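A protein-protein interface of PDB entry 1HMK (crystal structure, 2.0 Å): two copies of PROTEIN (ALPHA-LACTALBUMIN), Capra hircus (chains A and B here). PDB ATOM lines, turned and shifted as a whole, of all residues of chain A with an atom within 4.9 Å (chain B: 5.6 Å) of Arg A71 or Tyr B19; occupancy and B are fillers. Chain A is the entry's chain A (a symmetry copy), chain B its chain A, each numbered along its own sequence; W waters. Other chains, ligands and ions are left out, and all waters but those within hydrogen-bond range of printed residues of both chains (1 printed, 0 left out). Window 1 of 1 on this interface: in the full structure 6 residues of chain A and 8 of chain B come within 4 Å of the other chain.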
ATOM      1  N   LYS A  59      15.248  -8.263   1.988  1.00  0.00           N
ATOM      2  CA  LYS A  59      16.158  -9.201   2.620  1.00  0.00           C
ATOM      3  C   LYS A  59      15.397 -10.042   3.641  1.00  0.00           C
ATOM      4  O   LYS A  59      15.635 -11.243   3.784  1.00  0.00           O
ATOM      5  CB  LYS A  59      17.289  -8.441   3.317  1.00  0.00           C
ATOM      6  CG  LYS A  59      18.566  -9.244   3.496  1.00  0.00           C
ATOM      7  CD  LYS A  59      19.799  -8.364   3.315  1.00  0.00           C
ATOM      8  CE  LYS A  59      21.042  -9.198   3.019  1.00  0.00           C
ATOM      9  NZ  LYS A  59      21.481  -9.071   1.598  1.00  0.00           N
ATOM     10  N   ILE A  60      14.456  -9.405   4.328  1.00  0.00           N
ATOM     11  CA  ILE A  60      13.688 -10.075   5.361  1.00  0.00           C
ATOM     12  C   ILE A  60      12.181  -9.982   5.180  1.00  0.00           C
ATOM     13  O   ILE A  60      11.451 -10.923   5.490  1.00  0.00           O
ATOM     14  CB  ILE A  60      14.024  -9.465   6.756  1.00  0.00           C
ATOM     15  CG1 ILE A  60      15.507  -9.650   7.072  1.00  0.00           C
ATOM     16  CG2 ILE A  60      13.162 -10.095   7.841  1.00  0.00           C
ATOM     17  CD1 ILE A  60      15.898 -11.088   7.377  1.00  0.00           C
ATOM     18  N   HIS A  69      15.495 -15.401  -2.258  1.00  0.00           N
ATOM     19  CA  HIS A  69      15.792 -16.109  -1.017  1.00  0.00           C
ATOM     20  C   HIS A  69      15.456 -15.273   0.225  1.00  0.00           C
ATOM     21  O   HIS A  69      15.861 -15.603   1.339  1.00  0.00           O
ATOM     22  CB  HIS A  69      17.270 -16.504  -0.978  1.00  0.00           C
ATOM     23  CG  HIS A  69      17.621 -17.411   0.161  1.00  0.00           C
ATOM     24  ND1 HIS A  69      18.825 -17.337   0.828  1.00  0.00           N
ATOM     25  CD2 HIS A  69      16.920 -18.405   0.757  1.00  0.00           C
ATOM     26  CE1 HIS A  69      18.850 -18.248   1.785  1.00  0.00           C
ATOM     27  NE2 HIS A  69      17.706 -18.910   1.763  1.00  0.00           N
ATOM     28  N   SER A  70      14.725 -14.183   0.028  1.00  0.00           N
ATOM     29  CA  SER A  70      14.346 -13.327   1.142  1.00  0.00           C
ATOM     30  C   SER A  70      13.479 -14.117   2.127  1.00  0.00           C
ATOM     31  O   SER A  70      12.781 -15.054   1.737  1.00  0.00           O
ATOM     32  CB  SER A  70      13.581 -12.112   0.617  1.00  0.00           C
ATOM     33  OG  SER A  70      12.593 -11.690   1.538  1.00  0.00           O
ATOM     34  N   ARG A  71      13.538 -13.749   3.404  1.00  0.00           N
ATOM     35  CA  ARG A  71      12.740 -14.434   4.411  1.00  0.00           C
ATOM     36  C   ARG A  71      11.260 -14.252   4.094  1.00  0.00           C
ATOM     37  O   ARG A  71      10.422 -15.058   4.490  1.00  0.00           O
ATOM     38  CB  ARG A  71      13.057 -13.884   5.801  1.00  0.00           C
ATOM     39  CG  ARG A  71      13.570 -14.937   6.767  1.00  0.00           C
ATOM     40  CD  ARG A  71      13.173 -14.623   8.200  1.00  0.00           C
ATOM     41  NE  ARG A  71      12.702 -15.806   8.918  1.00  0.00           N
ATOM     42  CZ  ARG A  71      13.399 -16.930   9.064  1.00  0.00           C
ATOM     43  NH1 ARG A  71      14.615 -17.045   8.539  1.00  0.00           N
ATOM     44  NH2 ARG A  71      12.882 -17.942   9.743  1.00  0.00           N
ATOM     45  N   ASN A  72      10.950 -13.179   3.376  1.00  0.00           N
ATOM     46  CA  ASN A  72       9.580 -12.888   2.960  1.00  0.00           C
ATOM     47  C   ASN A  72       8.561 -12.950   4.094  1.00  0.00           C
ATOM     48  O   ASN A  72       7.470 -13.486   3.926  1.00  0.00           O
ATOM     49  CB  ASN A  72       9.167 -13.859   1.849  1.00  0.00           C
ATOM     50  CG  ASN A  72       7.970 -13.369   1.072  1.00  0.00           C
ATOM     51  OD1 ASN A  72       7.544 -12.224   1.232  1.00  0.00           O
ATOM     52  ND2 ASN A  72       7.415 -14.230   0.224  1.00  0.00           N
ATOM     53  N   ILE A  73       8.910 -12.382   5.241  1.00  0.00           N
ATOM     54  CA  ILE A  73       8.026 -12.385   6.401  1.00  0.00           C
ATOM     55  C   ILE A  73       6.629 -11.850   6.081  1.00  0.00           C
ATOM     56  O   ILE A  73       5.621 -12.377   6.562  1.00  0.00           O
ATOM     57  CB  ILE A  73       8.642 -11.559   7.544  1.00  0.00           C
ATOM     58  CG1 ILE A  73       9.845 -12.312   8.118  1.00  0.00           C
ATOM     59  CG2 ILE A  73       7.592 -11.282   8.617  1.00  0.00           C
ATOM     60  CD1 ILE A  73      10.422 -11.700   9.368  1.00  0.00           C
ATOM     61  N   LYS B  14      13.091 -23.733  14.953  1.00  0.00           N
ATOM     62  CA  LYS B  14      13.273 -22.305  15.201  1.00  0.00           C
ATOM     63  C   LYS B  14      13.611 -21.501  13.946  1.00  0.00           C
ATOM     64  O   LYS B  14      13.155 -20.368  13.779  1.00  0.00           O
ATOM     65  CB  LYS B  14      14.373 -22.097  16.244  1.00  0.00           C
ATOM     66  CG  LYS B  14      13.984 -21.168  17.381  1.00  0.00           C
ATOM     67  CD  LYS B  14      12.981 -21.819  18.330  1.00  0.00           C
ATOM     68  CE  LYS B  14      12.204 -20.768  19.114  1.00  0.00           C
ATOM     69  NZ  LYS B  14      12.372 -20.908  20.592  1.00  0.00           N
ATOM     70  N   ASP B  15      14.403 -22.092  13.058  1.00  0.00           N
ATOM     71  CA  ASP B  15      14.826 -21.420  11.831  1.00  0.00           C
ATOM     72  C   ASP B  15      13.736 -21.117  10.806  1.00  0.00           C
ATOM     73  O   ASP B  15      13.920 -20.267   9.933  1.00  0.00           O
ATOM     74  CB  ASP B  15      15.933 -22.228  11.155  1.00  0.00           C
ATOM     75  CG  ASP B  15      17.219 -21.452  11.041  1.00  0.00           C
ATOM     76  OD1 ASP B  15      17.158 -20.204  11.085  1.00  0.00           O
ATOM     77  OD2 ASP B  15      18.289 -22.086  10.911  1.00  0.00           O
ATOM     78  N   LEU B  16      12.608 -21.809  10.897  1.00  0.00           N
ATOM     79  CA  LEU B  16      11.515 -21.587   9.962  1.00  0.00           C
ATOM     80  C   LEU B  16      10.590 -20.464  10.433  1.00  0.00           C
ATOM     81  O   LEU B  16       9.702 -20.031   9.698  1.00  0.00           O
ATOM     82  CB  LEU B  16      10.709 -22.876   9.792  1.00  0.00           C
ATOM     83  CG  LEU B  16      11.350 -23.938   8.894  1.00  0.00           C
ATOM     84  CD1 LEU B  16      10.623 -25.267   9.026  1.00  0.00           C
ATOM     85  CD2 LEU B  16      11.314 -23.441   7.461  1.00  0.00           C
ATOM     86  N   LYS B  17      10.809 -19.996  11.658  1.00  0.00           N
ATOM     87  CA  LYS B  17       9.983 -18.939  12.238  1.00  0.00           C
ATOM     88  C   LYS B  17       9.728 -17.757  11.309  1.00  0.00           C
ATOM     89  O   LYS B  17      10.658 -17.086  10.861  1.00  0.00           O
ATOM     90  CB  LYS B  17      10.607 -18.439  13.541  1.00  0.00           C
ATOM     91  CG  LYS B  17       9.673 -17.586  14.373  1.00  0.00           C
ATOM     92  CD  LYS B  17      10.265 -17.308  15.731  1.00  0.00           C
ATOM     93  CE  LYS B  17      10.380 -15.821  15.962  1.00  0.00           C
ATOM     94  NZ  LYS B  17       9.305 -15.341  16.878  1.00  0.00           N
ATOM     95  N   ASP B  18       8.450 -17.525  11.026  1.00  0.00           N
ATOM     96  CA  ASP B  18       8.007 -16.436  10.169  1.00  0.00           C
ATOM     97  C   ASP B  18       8.492 -16.524   8.738  1.00  0.00           C
ATOM     98  O   ASP B  18       8.295 -15.590   7.957  1.00  0.00           O
ATOM     99  CB  ASP B  18       8.417 -15.086  10.766  1.00  0.00           C
ATOM    100  CG  ASP B  18       7.665 -14.772  12.039  1.00  0.00           C
ATOM    101  OD1 ASP B  18       6.519 -15.250  12.176  1.00  0.00           O
ATOM    102  OD2 ASP B  18       8.217 -14.060  12.901  1.00  0.00           O
ATOM    103  N   TYR B  19       9.122 -17.637   8.375  1.00  0.00           N
ATOM    104  CA  TYR B  19       9.579 -17.769   7.004  1.00  0.00           C
ATOM    105  C   TYR B  19       8.322 -17.785   6.155  1.00  0.00           C
ATOM    106  O   TYR B  19       7.406 -18.564   6.413  1.00  0.00           O
ATOM    107  CB  TYR B  19      10.366 -19.067   6.787  1.00  0.00           C
ATOM    108  CG  TYR B  19      10.908 -19.157   5.382  1.00  0.00           C
ATOM    109  CD1 TYR B  19      12.099 -18.521   5.036  1.00  0.00           C
ATOM    110  CD2 TYR B  19      10.185 -19.804   4.375  1.00  0.00           C
ATOM    111  CE1 TYR B  19      12.557 -18.518   3.725  1.00  0.00           C
ATOM    112  CE2 TYR B  19      10.630 -19.809   3.063  1.00  0.00           C
ATOM    113  CZ  TYR B  19      11.819 -19.161   2.743  1.00  0.00           C
ATOM    114  OH  TYR B  19      12.268 -19.154   1.442  1.00  0.00           O
ATOM    115  N   GLY B  20       8.270 -16.909   5.158  1.00  0.00           N
ATOM    116  CA  GLY B  20       7.108 -16.846   4.293  1.00  0.00           C
ATOM    117  C   GLY B  20       5.855 -16.435   5.039  1.00  0.00           C
ATOM    118  O   GLY B  20       4.744 -16.611   4.550  1.00  0.00           O
ATOM    119  N   GLY B  21       6.032 -15.879   6.232  1.00  0.00           N
ATOM    120  CA  GLY B  21       4.889 -15.446   7.009  1.00  0.00           C
ATOM    121  C   GLY B  21       4.283 -16.557   7.841  1.00  0.00           C
ATOM    122  O   GLY B  21       3.197 -16.392   8.399  1.00  0.00           O
ATOM    123  N   VAL B  22       4.974 -17.691   7.926  1.00  0.00           N
ATOM    124  CA  VAL B  22       4.473 -18.822   8.701  1.00  0.00           C
ATOM    125  C   VAL B  22       5.111 -18.812  10.079  1.00  0.00           C
ATOM    126  O   VAL B  22       6.324 -18.952  10.215  1.00  0.00           O
ATOM    127  CB  VAL B  22       4.774 -20.170   7.993  1.00  0.00           C
ATOM    128  CG1 VAL B  22       4.148 -21.329   8.774  1.00  0.00           C
ATOM    129  CG2 VAL B  22       4.214 -20.141   6.573  1.00  0.00           C
ATOM    130  N   TRP B  27       4.179 -24.022  12.057  1.00  0.00           N
ATOM    131  CA  TRP B  27       5.110 -25.048  11.559  1.00  0.00           C
ATOM    132  C   TRP B  27       5.075 -26.311  12.429  1.00  0.00           C
ATOM    133  O   TRP B  27       5.295 -27.419  11.939  1.00  0.00           O
ATOM    134  CB  TRP B  27       6.546 -24.516  11.537  1.00  0.00           C
ATOM    135  CG  TRP B  27       6.866 -23.635  10.370  1.00  0.00           C
ATOM    136  CD1 TRP B  27       7.172 -22.305  10.404  1.00  0.00           C
ATOM    137  CD2 TRP B  27       6.952 -24.031   9.000  1.00  0.00           C
ATOM    138  NE1 TRP B  27       7.446 -21.846   9.142  1.00  0.00           N
ATOM    139  CE2 TRP B  27       7.319 -22.886   8.257  1.00  0.00           C
ATOM    140  CE3 TRP B  27       6.755 -25.246   8.322  1.00  0.00           C
ATOM    141  CZ2 TRP B  27       7.497 -22.917   6.868  1.00  0.00           C
ATOM    142  CZ3 TRP B  27       6.932 -25.277   6.935  1.00  0.00           C
ATOM    143  CH2 TRP B  27       7.300 -24.117   6.226  1.00  0.00           C
ATOM    144  N   LYS B  94      11.663 -24.988   2.972  1.00  0.00           N
ATOM    145  CA  LYS B  94      11.564 -23.576   2.608  1.00  0.00           C
ATOM    146  C   LYS B  94      11.247 -23.439   1.117  1.00  0.00           C
ATOM    147  O   LYS B  94      10.499 -22.549   0.713  1.00  0.00           O
ATOM    148  CB  LYS B  94      12.867 -22.853   2.955  1.00  0.00           C
ATOM    149  CG  LYS B  94      12.985 -22.521   4.448  1.00  0.00           C
ATOM    150  CD  LYS B  94      14.234 -21.715   4.768  1.00  0.00           C
ATOM    151  CE  LYS B  94      14.388 -21.507   6.270  1.00  0.00           C
ATOM    152  NZ  LYS B  94      15.643 -20.782   6.631  1.00  0.00           N
ATOM    153  N   LYS B  95      11.810 -24.339   0.311  1.00  0.00           N
ATOM    154  CA  LYS B  95      11.588 -24.349  -1.137  1.00  0.00           C
ATOM    155  C   LYS B  95      10.167 -24.776  -1.484  1.00  0.00           C
ATOM    156  O   LYS B  95       9.534 -24.204  -2.372  1.00  0.00           O
ATOM    157  CB  LYS B  95      12.566 -25.307  -1.817  1.00  0.00           C
ATOM    158  CG  LYS B  95      13.977 -24.786  -1.925  1.00  0.00           C
ATOM    159  CD  LYS B  95      14.831 -25.765  -2.708  1.00  0.00           C
ATOM    160  CE  LYS B  95      16.245 -25.808  -2.171  1.00  0.00           C
ATOM    161  NZ  LYS B  95      16.878 -24.466  -2.228  1.00  0.00           N
ATOM    162  N   LEU B  97       7.512 -24.473   0.356  1.00  0.00           N
ATOM    163  CA  LEU B  97       6.616 -23.379   0.717  1.00  0.00           C
ATOM    164  C   LEU B  97       6.688 -22.303  -0.358  1.00  0.00           C
ATOM    165  O   LEU B  97       5.666 -21.876  -0.889  1.00  0.00           O
ATOM    166  CB  LEU B  97       7.011 -22.789   2.076  1.00  0.00           C
ATOM    167  CG  LEU B  97       6.049 -21.722   2.603  1.00  0.00           C
ATOM    168  CD1 LEU B  97       4.805 -22.392   3.173  1.00  0.00           C
ATOM    169  CD2 LEU B  97       6.749 -20.876   3.650  1.00  0.00           C
ATOM    170  N   ASP B  98       7.907 -21.881  -0.676  1.00  0.00           N
ATOM    171  CA  ASP B  98       8.140 -20.857  -1.687  1.00  0.00           C
ATOM    172  C   ASP B  98       7.505 -21.205  -3.024  1.00  0.00           C
ATOM    173  O   ASP B  98       6.977 -20.332  -3.709  1.00  0.00           O
ATOM    174  CB  ASP B  98       9.639 -20.658  -1.917  1.00  0.00           C
ATOM    175  CG  ASP B  98      10.292 -19.819  -0.844  1.00  0.00           C
ATOM    176  OD1 ASP B  98       9.567 -19.152  -0.076  1.00  0.00           O
ATOM    177  OD2 ASP B  98      11.538 -19.827  -0.771  1.00  0.00           O
HETATM  178  O   HOH W   1       7.873 -17.173   0.228  1.00  0.00           O
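Ser A70 touches none of the printed residues of chain B. Of the printed residues of chain A, Leu B16 touches Arg A71. Printed residues of chain A within 4 Å of Asp B18: Ile A73. Of the printed residues of chain A, Tyr B19 touches Arg A71 (3.8 Å). Printed residues of chain A within 4 Å of Gly B21: Asn A72 and Ile A73. The nearest residue of chain B that does not touch Arg A71 is Asp B18 (4.1 Å). The nearest printed residue of chain A that does not touch Tyr B19 is Ser A70 (4.0002 Å). The nearest printed residue of chain A that does not touch Asp B15 is His A69 (9.1 Å).
Water W1 bridges OD1 of Asp B98 (2.6 Å) and ND2 of Asn A72 (3.0 Å).
Among the printed residues, merely in contact across the chains: Ile A73 with Gly B21 (3.2 Å), Asn A72 with Gly B20 (3.4 Å), Arg A71 with Leu B16 (3.5 Å), Ile A73 with Asp B18 (3.6 Å), Asn A72 with Gly B21 (3.6 Å) and Arg A71 with Tyr B19 (3.8 Å).
O of Asp B15 is in hydrogen-bond range of NH2 of Arg A71. The guanidinium group of Arg A71 sits at hydrogen-bond distance from the backbone carbonyl oxygen of Lys B17 (2.6 Å). The backbone NH of Gly B20 lies within hydrogen-bond range of the backbone carbonyl oxygen of Arg A71.
Of the 14 printed residues of chain B, 7 touch a printed residue of chain A. Printed residues of chain A that touch a printed residue of chain B: Arg A71, Asn A72 and Ile A73. Hydrophobic or aromatic side chains of chain A within 4 Å of the printed part of chain B: Ile A73. Among the printed residues, no Asp or Glu carboxylate lies within 4 Å of a Lys or Arg side-chain nitrogen of the other chain.
No position is printed for both chains. Of the 9 pairs that touch across the chains among the printed residues, none has its exchanged pair printed and touching as well.
O of Ile A60 sits at hydrogen-bond distance from N of Ile A73 (2.9 Å). NE1 of Trp B27 lies within hydrogen-bond range of O of Leu B16 (2.9 Å). The side-chain hydroxyl (OG) of Ser A70 is in hydrogen-bond range of the backbone NH (N) of Asn A72 (2.9 Å). The side-chain hydroxyl (OH) of Tyr B19 sits at hydrogen-bond distance from the side-chain carboxylate (OD2) of Asp B98, at 2.4 Å. The backbone NH (N) of Arg A71 is in hydrogen-bond range of the backbone carbonyl oxygen (O) of Lys A59, 3.3 Å away. N of Asn A72 lies within hydrogen-bond range of O of Ile A60.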
